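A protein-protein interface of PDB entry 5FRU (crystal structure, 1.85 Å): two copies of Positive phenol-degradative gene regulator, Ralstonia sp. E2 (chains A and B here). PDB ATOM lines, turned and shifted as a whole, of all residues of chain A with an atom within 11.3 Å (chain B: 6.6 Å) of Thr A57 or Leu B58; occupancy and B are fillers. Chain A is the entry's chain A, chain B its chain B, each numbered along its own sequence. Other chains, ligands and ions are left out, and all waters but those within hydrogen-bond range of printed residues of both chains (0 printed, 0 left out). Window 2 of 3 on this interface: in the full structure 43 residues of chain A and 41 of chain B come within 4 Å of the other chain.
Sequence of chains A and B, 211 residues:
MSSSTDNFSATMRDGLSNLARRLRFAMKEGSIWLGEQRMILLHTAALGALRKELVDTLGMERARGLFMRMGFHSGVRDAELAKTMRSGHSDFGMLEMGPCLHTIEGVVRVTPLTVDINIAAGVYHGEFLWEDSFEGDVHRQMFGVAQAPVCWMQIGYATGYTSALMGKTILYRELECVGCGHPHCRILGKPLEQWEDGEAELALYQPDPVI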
ATOM      1  N   GLY A  48      12.898 -31.010  -3.543  1.00  0.00           N
ATOM      2  CA  GLY A  48      14.021 -30.241  -4.056  1.00  0.00           C
ATOM      3  C   GLY A  48      14.384 -30.622  -5.478  1.00  0.00           C
ATOM      4  O   GLY A  48      14.581 -29.758  -6.332  1.00  0.00           O
ATOM      5  N   ALA A  49      14.447 -31.919  -5.751  1.00  0.00           N
ATOM      6  CA  ALA A  49      14.825 -32.371  -7.085  1.00  0.00           C
ATOM      7  C   ALA A  49      13.788 -31.953  -8.105  1.00  0.00           C
ATOM      8  O   ALA A  49      14.127 -31.507  -9.200  1.00  0.00           O
ATOM      9  CB  ALA A  49      15.021 -33.883  -7.105  1.00  0.00           C
ATOM     10  N   LEU A  50      12.518 -32.087  -7.736  1.00  0.00           N
ATOM     11  CA  LEU A  50      11.423 -31.605  -8.562  1.00  0.00           C
ATOM     12  C   LEU A  50      11.504 -30.107  -8.827  1.00  0.00           C
ATOM     13  O   LEU A  50      11.322 -29.650  -9.957  1.00  0.00           O
ATOM     14  CB  LEU A  50      10.085 -31.905  -7.905  1.00  0.00           C
ATOM     15  CG  LEU A  50       8.948 -31.273  -8.703  1.00  0.00           C
ATOM     16  CD1 LEU A  50       8.871 -31.857 -10.119  1.00  0.00           C
ATOM     17  CD2 LEU A  50       7.633 -31.430  -7.960  1.00  0.00           C
ATOM     18  N   ARG A  51      11.757 -29.351  -7.771  1.00  0.00           N
ATOM     19  CA  ARG A  51      11.882 -27.907  -7.897  1.00  0.00           C
ATOM     20  C   ARG A  51      12.975 -27.535  -8.896  1.00  0.00           C
ATOM     21  O   ARG A  51      12.782 -26.661  -9.730  1.00  0.00           O
ATOM     22  CB  ARG A  51      12.177 -27.268  -6.538  1.00  0.00           C
ATOM     23  CG  ARG A  51      12.633 -25.810  -6.643  1.00  0.00           C
ATOM     24  CD  ARG A  51      12.763 -25.157  -5.274  1.00  0.00           C
ATOM     25  NE  ARG A  51      11.468 -25.169  -4.640  1.00  0.00           N
ATOM     26  CZ  ARG A  51      10.875 -24.133  -4.066  1.00  0.00           C
ATOM     27  NH1 ARG A  51      11.455 -22.937  -3.973  1.00  0.00           N
ATOM     28  NH2 ARG A  51       9.684 -24.335  -3.564  1.00  0.00           N
ATOM     29  N   LYS A  52      14.118 -28.206  -8.826  1.00  0.00           N
ATOM     30  CA  LYS A  52      15.223 -27.837  -9.717  1.00  0.00           C
ATOM     31  C   LYS A  52      14.901 -28.130 -11.178  1.00  0.00           C
ATOM     32  O   LYS A  52      15.188 -27.317 -12.048  1.00  0.00           O
ATOM     33  CB  LYS A  52      16.523 -28.540  -9.336  1.00  0.00           C
ATOM     34  CG  LYS A  52      17.656 -28.145 -10.274  1.00  0.00           C
ATOM     35  CD  LYS A  52      18.980 -28.788  -9.918  1.00  0.00           C
ATOM     36  CE  LYS A  52      20.089 -28.157 -10.747  1.00  0.00           C
ATOM     37  NZ  LYS A  52      19.685 -28.020 -12.181  1.00  0.00           N
ATOM     38  N   GLU A  53      14.292 -29.280 -11.448  1.00  0.00           N
ATOM     39  CA  GLU A  53      13.883 -29.607 -12.814  1.00  0.00           C
ATOM     40  C   GLU A  53      12.808 -28.674 -13.383  1.00  0.00           C
ATOM     41  O   GLU A  53      12.851 -28.314 -14.560  1.00  0.00           O
ATOM     42  CB  GLU A  53      13.398 -31.050 -12.871  1.00  0.00           C
ATOM     43  CG  GLU A  53      14.484 -32.027 -12.485  1.00  0.00           C
ATOM     44  CD  GLU A  53      14.329 -33.367 -13.157  1.00  0.00           C
ATOM     45  OE1 GLU A  53      14.352 -33.425 -14.408  1.00  0.00           O
ATOM     46  OE2 GLU A  53      14.183 -34.364 -12.422  1.00  0.00           O
ATOM     47  N   LEU A  54      11.849 -28.274 -12.556  1.00  0.00           N
ATOM     48  CA  LEU A  54      10.811 -27.364 -13.024  1.00  0.00           C
ATOM     49  C   LEU A  54      11.376 -25.991 -13.375  1.00  0.00           C
ATOM     50  O   LEU A  54      11.024 -25.408 -14.406  1.00  0.00           O
ATOM     51  CB  LEU A  54       9.714 -27.216 -11.976  1.00  0.00           C
ATOM     52  CG  LEU A  54       8.913 -28.488 -11.696  1.00  0.00           C
ATOM     53  CD1 LEU A  54       7.693 -28.175 -10.846  1.00  0.00           C
ATOM     54  CD2 LEU A  54       8.517 -29.192 -12.994  1.00  0.00           C
ATOM     55  N   VAL A  55      12.236 -25.467 -12.508  1.00  0.00           N
ATOM     56  CA  VAL A  55      12.872 -24.181 -12.763  1.00  0.00           C
ATOM     57  C   VAL A  55      13.730 -24.282 -14.020  1.00  0.00           C
ATOM     58  O   VAL A  55      13.794 -23.351 -14.810  1.00  0.00           O
ATOM     59  CB  VAL A  55      13.744 -23.712 -11.564  1.00  0.00           C
ATOM     60  CG1 VAL A  55      14.665 -22.578 -11.968  1.00  0.00           C
ATOM     61  CG2 VAL A  55      12.870 -23.279 -10.408  1.00  0.00           C
ATOM     62  N   ASP A  56      14.380 -25.420 -14.217  1.00  0.00           N
ATOM     63  CA  ASP A  56      15.257 -25.566 -15.371  1.00  0.00           C
ATOM     64  C   ASP A  56      14.479 -25.699 -16.671  1.00  0.00           C
ATOM     65  O   ASP A  56      14.921 -25.234 -17.722  1.00  0.00           O
ATOM     66  CB  ASP A  56      16.176 -26.762 -15.192  1.00  0.00           C
ATOM     67  CG  ASP A  56      17.247 -26.509 -14.153  1.00  0.00           C
ATOM     68  OD1 ASP A  56      17.314 -25.363 -13.668  1.00  0.00           O
ATOM     69  OD2 ASP A  56      18.005 -27.438 -13.814  1.00  0.00           O
ATOM     70  N   THR A  57      13.317 -26.332 -16.594  1.00  0.00           N
ATOM     71  CA  THR A  57      12.506 -26.570 -17.775  1.00  0.00           C
ATOM     72  C   THR A  57      11.540 -25.404 -18.018  1.00  0.00           C
ATOM     73  O   THR A  57      11.433 -24.896 -19.140  1.00  0.00           O
ATOM     74  CB  THR A  57      11.722 -27.894 -17.643  1.00  0.00           C
ATOM     75  OG1 THR A  57      12.645 -28.960 -17.389  1.00  0.00           O
ATOM     76  CG2 THR A  57      10.945 -28.202 -18.922  1.00  0.00           C
ATOM     77  N   LEU A  58      10.861 -24.973 -16.956  1.00  0.00           N
ATOM     78  CA  LEU A  58       9.783 -24.004 -17.073  1.00  0.00           C
ATOM     79  C   LEU A  58      10.220 -22.609 -16.654  1.00  0.00           C
ATOM     80  O   LEU A  58       9.416 -21.695 -16.642  1.00  0.00           O
ATOM     81  CB  LEU A  58       8.580 -24.408 -16.216  1.00  0.00           C
ATOM     82  CG  LEU A  58       8.165 -25.862 -15.997  1.00  0.00           C
ATOM     83  CD1 LEU A  58       7.026 -25.864 -15.025  1.00  0.00           C
ATOM     84  CD2 LEU A  58       7.753 -26.555 -17.267  1.00  0.00           C
ATOM     85  N   GLY A  59      11.481 -22.443 -16.288  1.00  0.00           N
ATOM     86  CA  GLY A  59      11.939 -21.164 -15.777  1.00  0.00           C
ATOM     87  C   GLY A  59      11.388 -20.874 -14.391  1.00  0.00           C
ATOM     88  O   GLY A  59      10.409 -21.486 -13.953  1.00  0.00           O
ATOM     89  N   MET A  60      12.013 -19.922 -13.711  1.00  0.00           N
ATOM     90  CA  MET A  60      11.698 -19.584 -12.326  1.00  0.00           C
ATOM     91  C   MET A  60      10.246 -19.136 -12.125  1.00  0.00           C
ATOM     92  O   MET A  60       9.605 -19.512 -11.146  1.00  0.00           O
ATOM     93  CB  MET A  60      12.657 -18.489 -11.845  1.00  0.00           C
ATOM     94  CG  MET A  60      12.678 -18.254 -10.351  1.00  0.00           C
ATOM     95  SD  MET A  60      13.623 -19.484  -9.425  1.00  0.00           S
ATOM     96  CE  MET A  60      15.309 -19.133  -9.921  1.00  0.00           C
ATOM     97  N   GLU A  61       9.731 -18.346 -13.062  1.00  0.00           N
ATOM     98  CA  GLU A  61       8.394 -17.773 -12.947  1.00  0.00           C
ATOM     99  C   GLU A  61       7.263 -18.809 -12.935  1.00  0.00           C
ATOM    100  O   GLU A  61       6.329 -18.707 -12.138  1.00  0.00           O
ATOM    101  CB  GLU A  61       8.152 -16.776 -14.085  1.00  0.00           C
ATOM    102  CG  GLU A  61       9.059 -15.550 -14.068  1.00  0.00           C
ATOM    103  CD  GLU A  61      10.381 -15.764 -14.800  1.00  0.00           C
ATOM    104  OE1 GLU A  61      10.664 -16.910 -15.223  1.00  0.00           O
ATOM    105  OE2 GLU A  61      11.142 -14.780 -14.949  1.00  0.00           O
ATOM    106  N   ARG A  62       7.329 -19.787 -13.830  1.00  0.00           N
ATOM    107  CA  ARG A  62       6.312 -20.831 -13.875  1.00  0.00           C
ATOM    108  C   ARG A  62       6.438 -21.817 -12.747  1.00  0.00           C
ATOM    109  O   ARG A  62       5.432 -22.271 -12.213  1.00  0.00           O
ATOM    110  CB  ARG A  62       6.369 -21.594 -15.185  1.00  0.00           C
ATOM    111  CG  ARG A  62       5.797 -20.788 -16.267  1.00  0.00           C
ATOM    112  CD  ARG A  62       5.055 -21.593 -17.289  1.00  0.00           C
ATOM    113  NE  ARG A  62       4.564 -20.635 -18.266  1.00  0.00           N
ATOM    114  CZ  ARG A  62       3.369 -20.668 -18.845  1.00  0.00           C
ATOM    115  NH1 ARG A  62       2.517 -21.663 -18.618  1.00  0.00           N
ATOM    116  NH2 ARG A  62       3.044 -19.708 -19.692  1.00  0.00           N
ATOM    117  N   ALA A  63       7.673 -22.164 -12.400  1.00  0.00           N
ATOM    118  CA  ALA A  63       7.902 -23.071 -11.285  1.00  0.00           C
ATOM    119  C   ALA A  63       7.239 -22.482 -10.056  1.00  0.00           C
ATOM    120  O   ALA A  63       6.620 -23.193  -9.272  1.00  0.00           O
ATOM    121  CB  ALA A  63       9.393 -23.288 -11.049  1.00  0.00           C
ATOM    122  N   ARG A  64       7.359 -21.168  -9.909  1.00  0.00           N
ATOM    123  CA  ARG A  64       6.811 -20.482  -8.748  1.00  0.00           C
ATOM    124  C   ARG A  64       5.286 -20.605  -8.719  1.00  0.00           C
ATOM    125  O   ARG A  64       4.707 -20.946  -7.685  1.00  0.00           O
ATOM    126  CB  ARG A  64       7.241 -19.015  -8.747  1.00  0.00           C
ATOM    127  CG  ARG A  64       6.621 -18.182  -7.642  1.00  0.00           C
ATOM    128  CD  ARG A  64       7.279 -16.804  -7.556  1.00  0.00           C
ATOM    129  NE  ARG A  64       6.470 -15.858  -6.794  1.00  0.00           N
ATOM    130  CZ  ARG A  64       5.954 -14.740  -7.296  1.00  0.00           C
ATOM    131  NH1 ARG A  64       6.176 -14.415  -8.564  1.00  0.00           N
ATOM    132  NH2 ARG A  64       5.224 -13.940  -6.530  1.00  0.00           N
ATOM    133  N   LEU A  66       3.488 -22.937 -10.190  1.00  0.00           N
ATOM    134  CA  LEU A  66       3.159 -24.337  -9.944  1.00  0.00           C
ATOM    135  C   LEU A  66       3.167 -24.678  -8.459  1.00  0.00           C
ATOM    136  O   LEU A  66       2.242 -25.327  -7.960  1.00  0.00           O
ATOM    137  CB  LEU A  66       4.137 -25.268 -10.666  1.00  0.00           C
ATOM    138  CG  LEU A  66       3.855 -25.620 -12.121  1.00  0.00           C
ATOM    139  CD1 LEU A  66       4.843 -26.669 -12.531  1.00  0.00           C
ATOM    140  CD2 LEU A  66       2.447 -26.150 -12.271  1.00  0.00           C
ATOM    141  N   PHE A  67       4.222 -24.252  -7.767  1.00  0.00           N
ATOM    142  CA  PHE A  67       4.364 -24.536  -6.344  1.00  0.00           C
ATOM    143  C   PHE A  67       3.338 -23.770  -5.522  1.00  0.00           C
ATOM    144  O   PHE A  67       2.788 -24.292  -4.560  1.00  0.00           O
ATOM    145  CB  PHE A  67       5.790 -24.223  -5.874  1.00  0.00           C
ATOM    146  CG  PHE A  67       6.749 -25.368  -6.094  1.00  0.00           C
ATOM    147  CD1 PHE A  67       7.425 -25.501  -7.292  1.00  0.00           C
ATOM    148  CD2 PHE A  67       6.938 -26.322  -5.116  1.00  0.00           C
ATOM    149  CE1 PHE A  67       8.288 -26.570  -7.504  1.00  0.00           C
ATOM    150  CE2 PHE A  67       7.802 -27.394  -5.316  1.00  0.00           C
ATOM    151  CZ  PHE A  67       8.471 -27.515  -6.514  1.00  0.00           C
ATOM    152  N   ARG A  69       0.369 -22.926  -6.471  1.00  0.00           N
ATOM    153  CA  ARG A  69      -0.934 -23.576  -6.639  1.00  0.00           C
ATOM    154  C   ARG A  69      -1.010 -24.879  -5.844  1.00  0.00           C
ATOM    155  O   ARG A  69      -2.063 -25.215  -5.306  1.00  0.00           O
ATOM    156  CB  ARG A  69      -1.223 -23.838  -8.124  1.00  0.00           C
ATOM    157  CG  ARG A  69      -1.568 -22.578  -8.925  1.00  0.00           C
ATOM    158  CD  ARG A  69      -1.482 -22.832 -10.428  1.00  0.00           C
ATOM    159  NE  ARG A  69      -0.548 -21.906 -11.063  1.00  0.00           N
ATOM    160  CZ  ARG A  69       0.339 -22.247 -11.989  1.00  0.00           C
ATOM    161  NH1 ARG A  69       0.425 -23.498 -12.402  1.00  0.00           N
ATOM    162  NH2 ARG A  69       1.143 -21.331 -12.506  1.00  0.00           N
ATOM    163  N   PHE A 143      19.821 -24.354  -5.029  1.00  0.00           N
ATOM    164  CA  PHE A 143      20.094 -23.135  -5.784  1.00  0.00           C
ATOM    165  C   PHE A 143      21.093 -22.190  -5.131  1.00  0.00           C
ATOM    166  O   PHE A 143      21.495 -21.215  -5.758  1.00  0.00           O
ATOM    167  CB  PHE A 143      18.804 -22.333  -6.009  1.00  0.00           C
ATOM    168  CG  PHE A 143      17.758 -23.053  -6.796  1.00  0.00           C
ATOM    169  CD1 PHE A 143      17.807 -23.081  -8.179  1.00  0.00           C
ATOM    170  CD2 PHE A 143      16.705 -23.677  -6.150  1.00  0.00           C
ATOM    171  CE1 PHE A 143      16.826 -23.735  -8.906  1.00  0.00           C
ATOM    172  CE2 PHE A 143      15.727 -24.325  -6.862  1.00  0.00           C
ATOM    173  CZ  PHE A 143      15.782 -24.358  -8.243  1.00  0.00           C
ATOM    174  N   TRP A 152       7.431 -20.518  -1.997  1.00  0.00           N
ATOM    175  CA  TRP A 152       6.282 -20.488  -2.885  1.00  0.00           C
ATOM    176  C   TRP A 152       5.128 -21.368  -2.388  1.00  0.00           C
ATOM    177  O   TRP A 152       3.981 -20.900  -2.273  1.00  0.00           O
ATOM    178  CB  TRP A 152       6.709 -20.932  -4.285  1.00  0.00           C
ATOM    179  CG  TRP A 152       7.881 -20.187  -4.839  1.00  0.00           C
ATOM    180  CD1 TRP A 152       8.204 -18.868  -4.621  1.00  0.00           C
ATOM    181  CD2 TRP A 152       8.885 -20.705  -5.716  1.00  0.00           C
ATOM    182  NE1 TRP A 152       9.352 -18.543  -5.310  1.00  0.00           N
ATOM    183  CE2 TRP A 152       9.793 -19.655  -5.984  1.00  0.00           C
ATOM    184  CE3 TRP A 152       9.115 -21.960  -6.295  1.00  0.00           C
ATOM    185  CZ2 TRP A 152      10.901 -19.821  -6.812  1.00  0.00           C
ATOM    186  CZ3 TRP A 152      10.228 -22.123  -7.117  1.00  0.00           C
ATOM    187  CH2 TRP A 152      11.099 -21.057  -7.369  1.00  0.00           C
ATOM    188  N   ASP A 208      -3.057 -23.528 -16.250  1.00  0.00           N
ATOM    189  CA  ASP A 208      -2.753 -23.159 -17.628  1.00  0.00           C
ATOM    190  C   ASP A 208      -1.714 -22.044 -17.683  1.00  0.00           C
ATOM    191  O   ASP A 208      -0.583 -22.258 -18.120  1.00  0.00           O
ATOM    192  CB  ASP A 208      -4.025 -22.728 -18.360  1.00  0.00           C
ATOM    193  CG  ASP A 208      -4.892 -23.905 -18.764  1.00  0.00           C
ATOM    194  OD1 ASP A 208      -4.417 -25.056 -18.668  1.00  0.00           O
ATOM    195  OD2 ASP A 208      -6.049 -23.679 -19.176  1.00  0.00           O
ATOM    196  N   GLU B  53      -1.282 -30.540 -13.565  1.00  0.00           N
ATOM    197  CA  GLU B  53      -0.694 -29.393 -14.234  1.00  0.00           C
ATOM    198  C   GLU B  53       0.526 -29.787 -15.045  1.00  0.00           C
ATOM    199  O   GLU B  53       0.706 -29.288 -16.147  1.00  0.00           O
ATOM    200  CB  GLU B  53      -0.331 -28.298 -13.228  1.00  0.00           C
ATOM    201  CG  GLU B  53      -1.539 -27.714 -12.527  1.00  0.00           C
ATOM    202  CD  GLU B  53      -1.312 -26.276 -12.058  1.00  0.00           C
ATOM    203  OE1 GLU B  53      -0.985 -25.413 -12.901  1.00  0.00           O
ATOM    204  OE2 GLU B  53      -1.460 -26.014 -10.846  1.00  0.00           O
ATOM    205  N   LEU B  54       1.355 -30.684 -14.513  1.00  0.00           N
ATOM    206  CA  LEU B  54       2.552 -31.119 -15.230  1.00  0.00           C
ATOM    207  C   LEU B  54       2.185 -31.907 -16.467  1.00  0.00           C
ATOM    208  O   LEU B  54       2.777 -31.706 -17.522  1.00  0.00           O
ATOM    209  CB  LEU B  54       3.458 -31.955 -14.332  1.00  0.00           C
ATOM    210  CG  LEU B  54       4.114 -31.140 -13.225  1.00  0.00           C
ATOM    211  CD1 LEU B  54       5.000 -32.028 -12.385  1.00  0.00           C
ATOM    212  CD2 LEU B  54       4.903 -29.963 -13.819  1.00  0.00           C
ATOM    213  N   VAL B  55       1.193 -32.784 -16.354  1.00  0.00           N
ATOM    214  CA  VAL B  55       0.724 -33.505 -17.530  1.00  0.00           C
ATOM    215  C   VAL B  55       0.128 -32.526 -18.562  1.00  0.00           C
ATOM    216  O   VAL B  55       0.441 -32.621 -19.753  1.00  0.00           O
ATOM    217  CB  VAL B  55      -0.302 -34.603 -17.159  1.00  0.00           C
ATOM    218  CG1 VAL B  55      -0.888 -35.227 -18.412  1.00  0.00           C
ATOM    219  CG2 VAL B  55       0.364 -35.684 -16.300  1.00  0.00           C
ATOM    220  N   ASP B  56      -0.687 -31.570 -18.111  1.00  0.00           N
ATOM    221  CA  ASP B  56      -1.243 -30.551 -19.020  1.00  0.00           C
ATOM    222  C   ASP B  56      -0.167 -29.687 -19.679  1.00  0.00           C
ATOM    223  O   ASP B  56      -0.290 -29.303 -20.846  1.00  0.00           O
ATOM    224  CB  ASP B  56      -2.216 -29.621 -18.285  1.00  0.00           C
ATOM    225  CG  ASP B  56      -3.480 -30.322 -17.843  1.00  0.00           C
ATOM    226  OD1 ASP B  56      -3.696 -31.484 -18.251  1.00  0.00           O
ATOM    227  OD2 ASP B  56      -4.251 -29.708 -17.069  1.00  0.00           O
ATOM    228  N   THR B  57       0.877 -29.348 -18.937  1.00  0.00           N
ATOM    229  CA  THR B  57       1.896 -28.465 -19.501  1.00  0.00           C
ATOM    230  C   THR B  57       3.035 -29.192 -20.210  1.00  0.00           C
ATOM    231  O   THR B  57       3.602 -28.651 -21.148  1.00  0.00           O
ATOM    232  CB  THR B  57       2.504 -27.529 -18.426  1.00  0.00           C
ATOM    233  OG1 THR B  57       3.307 -28.288 -17.517  1.00  0.00           O
ATOM    234  CG2 THR B  57       1.404 -26.813 -17.664  1.00  0.00           C
ATOM    235  N   LEU B  58       3.391 -30.406 -19.797  1.00  0.00           N
ATOM    236  CA  LEU B  58       4.578 -31.017 -20.392  1.00  0.00           C
ATOM    237  C   LEU B  58       4.275 -32.292 -21.147  1.00  0.00           C
ATOM    238  O   LEU B  58       5.118 -32.788 -21.885  1.00  0.00           O
ATOM    239  CB  LEU B  58       5.627 -31.321 -19.321  1.00  0.00           C
ATOM    240  CG  LEU B  58       6.289 -30.139 -18.627  1.00  0.00           C
ATOM    241  CD1 LEU B  58       6.976 -30.627 -17.374  1.00  0.00           C
ATOM    242  CD2 LEU B  58       7.261 -29.412 -19.546  1.00  0.00           C
ATOM    243  N   GLY B  59       3.088 -32.837 -20.932  1.00  0.00           N
ATOM    244  CA  GLY B  59       2.720 -34.095 -21.552  1.00  0.00           C
ATOM    245  C   GLY B  59       3.068 -35.245 -20.631  1.00  0.00           C
ATOM    246  O   GLY B  59       3.954 -35.123 -19.774  1.00  0.00           O
ATOM    247  N   MET B  60       2.366 -36.356 -20.824  1.00  0.00           N
ATOM    248  CA  MET B  60       2.486 -37.549 -19.996  1.00  0.00           C
ATOM    249  C   MET B  60       3.908 -38.066 -19.893  1.00  0.00           C
ATOM    250  O   MET B  60       4.354 -38.459 -18.817  1.00  0.00           O
ATOM    251  CB  MET B  60       1.594 -38.656 -20.561  1.00  0.00           C
ATOM    252  CG  MET B  60       1.135 -39.696 -19.562  1.00  0.00           C
ATOM    253  SD  MET B  60      -0.201 -39.066 -18.532  1.00  0.00           S
ATOM    254  CE  MET B  60      -1.373 -38.555 -19.773  1.00  0.00           C
ATOM    255  N   GLU B  61       4.612 -38.104 -21.019  1.00  0.00           N
ATOM    256  CA  GLU B  61       5.951 -38.688 -21.058  1.00  0.00           C
ATOM    257  C   GLU B  61       6.920 -37.894 -20.195  1.00  0.00           C
ATOM    258  O   GLU B  61       7.659 -38.469 -19.399  1.00  0.00           O
ATOM    259  CB  GLU B  61       6.480 -38.767 -22.496  1.00  0.00           C
ATOM    260  CG  GLU B  61       5.558 -39.467 -23.482  1.00  0.00           C
ATOM    261  CD  GLU B  61       4.315 -38.655 -23.825  1.00  0.00           C
ATOM    262  OE1 GLU B  61       4.374 -37.406 -23.762  1.00  0.00           O
ATOM    263  OE2 GLU B  61       3.270 -39.273 -24.131  1.00  0.00           O
ATOM    264  N   ARG B  62       6.913 -36.569 -20.332  1.00  0.00           N
ATOM    265  CA  ARG B  62       7.850 -35.757 -19.564  1.00  0.00           C
ATOM    266  C   ARG B  62       7.479 -35.735 -18.086  1.00  0.00           C
ATOM    267  O   ARG B  62       8.357 -35.774 -17.228  1.00  0.00           O
ATOM    268  CB  ARG B  62       7.914 -34.330 -20.107  1.00  0.00           C
ATOM    269  CG  ARG B  62       8.499 -34.241 -21.505  1.00  0.00           C
ATOM    270  CD  ARG B  62       8.468 -32.812 -22.047  1.00  0.00           C
ATOM    271  NE  ARG B  62       8.936 -32.771 -23.431  1.00  0.00           N
ATOM    272  CZ  ARG B  62       8.140 -32.601 -24.483  1.00  0.00           C
ATOM    273  NH1 ARG B  62       6.831 -32.435 -24.316  1.00  0.00           N
ATOM    274  NH2 ARG B  62       8.656 -32.587 -25.703  1.00  0.00           N
ATOM    275  N   ALA B  63       6.183 -35.684 -17.798  1.00  0.00           N
ATOM    276  CA  ALA B  63       5.709 -35.756 -16.417  1.00  0.00           C
ATOM    277  C   ALA B  63       6.163 -37.050 -15.767  1.00  0.00           C
ATOM    278  O   ALA B  63       6.544 -37.058 -14.594  1.00  0.00           O
ATOM    279  CB  ALA B  63       4.193 -35.638 -16.357  1.00  0.00           C
ATOM    280  N   LEU B  66       9.793 -36.761 -14.597  1.00  0.00           N
ATOM    281  CA  LEU B  66       9.897 -35.887 -13.426  1.00  0.00           C
ATOM    282  C   LEU B  66       9.556 -36.622 -12.138  1.00  0.00           C
ATOM    283  O   LEU B  66      10.297 -36.539 -11.164  1.00  0.00           O
ATOM    284  CB  LEU B  66       8.976 -34.667 -13.561  1.00  0.00           C
ATOM    285  CG  LEU B  66       9.455 -33.668 -14.602  1.00  0.00           C
ATOM    286  CD1 LEU B  66       8.399 -32.616 -14.853  1.00  0.00           C
ATOM    287  CD2 LEU B  66      10.720 -33.016 -14.106  1.00  0.00           C
ATOM    288  N   ASP B 208      17.113 -34.235 -18.735  1.00  0.00           N
ATOM    289  CA  ASP B 208      16.604 -34.335 -20.097  1.00  0.00           C
ATOM    290  C   ASP B 208      17.552 -33.674 -21.091  1.00  0.00           C
ATOM    291  O   ASP B 208      17.621 -32.448 -21.177  1.00  0.00           O
ATOM    292  CB  ASP B 208      15.213 -33.704 -20.198  1.00  0.00           C
ATOM    293  CG  ASP B 208      14.149 -34.527 -19.501  1.00  0.00           C
ATOM    294  OD1 ASP B 208      14.415 -35.706 -19.189  1.00  0.00           O
ATOM    295  OD2 ASP B 208      13.043 -33.995 -19.265  1.00  0.00           O
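The guanidinium group (NH1) of Arg A69 is in salt-bridge range of the side-chain carboxylate (OE1) of Glu B53.
The backbone carbonyl oxygen of Leu B58 lies within hydrogen-bond range of the guanidinium group of Arg B62, at 3.0 Å.
OG1 of Thr B57 sits at hydrogen-bond distance from O of Leu B54.
OG1 of Thr A57 lies within hydrogen-bond range of O of Glu A53 (2.9 Å).
O of Glu B53 lies close to OG1 of Thr B57 (3.1 Å).
Among the printed residues, merely in contact across the chains: Glu A53 with Leu B66, Leu A54 with Leu B54, Leu A54 with Leu B66, Thr A57 with Leu B58, Leu A58 with Leu B58, Leu A66 with Glu B53 and Leu A66 with Leu B54.
Of the printed residues of chain B, Glu A53 touches Leu B66 (3.5 Å).
Of the printed residues of chain B, Thr A57 touches Leu B58.
Of the printed residues of chain B, Leu A58 touches Leu B58.
Glu A61 touches none of the printed residues of chain B.
Printed residues of chain B within 4 Å of Arg A69: Glu B53 (2.4 Å).
Of the printed residues of chain A, Glu B53 touches Leu A66 and Arg A69.
Of chain A, only Leu A54 and Leu A66 come within 4 Å of Leu B54.
No residue of chain A comes within 4 Å of Thr B57.
Printed residues of chain A within 4 Å of Leu B58: Thr A57 and Leu A58.
No residue of chain A comes within 4 Å of Gly B59.
No residue of chain A comes within 4 Å of Glu B61.
No residue of chain A comes within 4 Å of Arg B62.
No residue of chain A comes within 4 Å of Ala B63.
Printed residues of chain A within 4 Å of Leu B66: Glu A53 and Leu A54.
Of the 13 printed residues of chain B, 4 touch a printed residue of chain A.
Printed residues of chain A that touch a printed residue of chain B: Glu A53, Leu A54, Thr A57, Leu A58, Leu A66 and Arg A69.
Among the printed residues, Asp or Glu carboxylates within 4 Å of a Lys or Arg side-chain nitrogen of the other chain: Arg A69 with Glu B53 (2.4 Å).
Glu A53 touches Leu B66, and with the chains exchanged Leu A66 touches Glu B53.
Leu A54 touches its own counterpart, Leu B54.
Leu A54 touches Leu B66, and with the chains exchanged Leu A66 touches Leu B54.
Thr A57 touches Leu B58, but with the chains exchanged Leu A58 does not touch Thr B57 (4.8 Å).
13 positions are printed for both chains.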
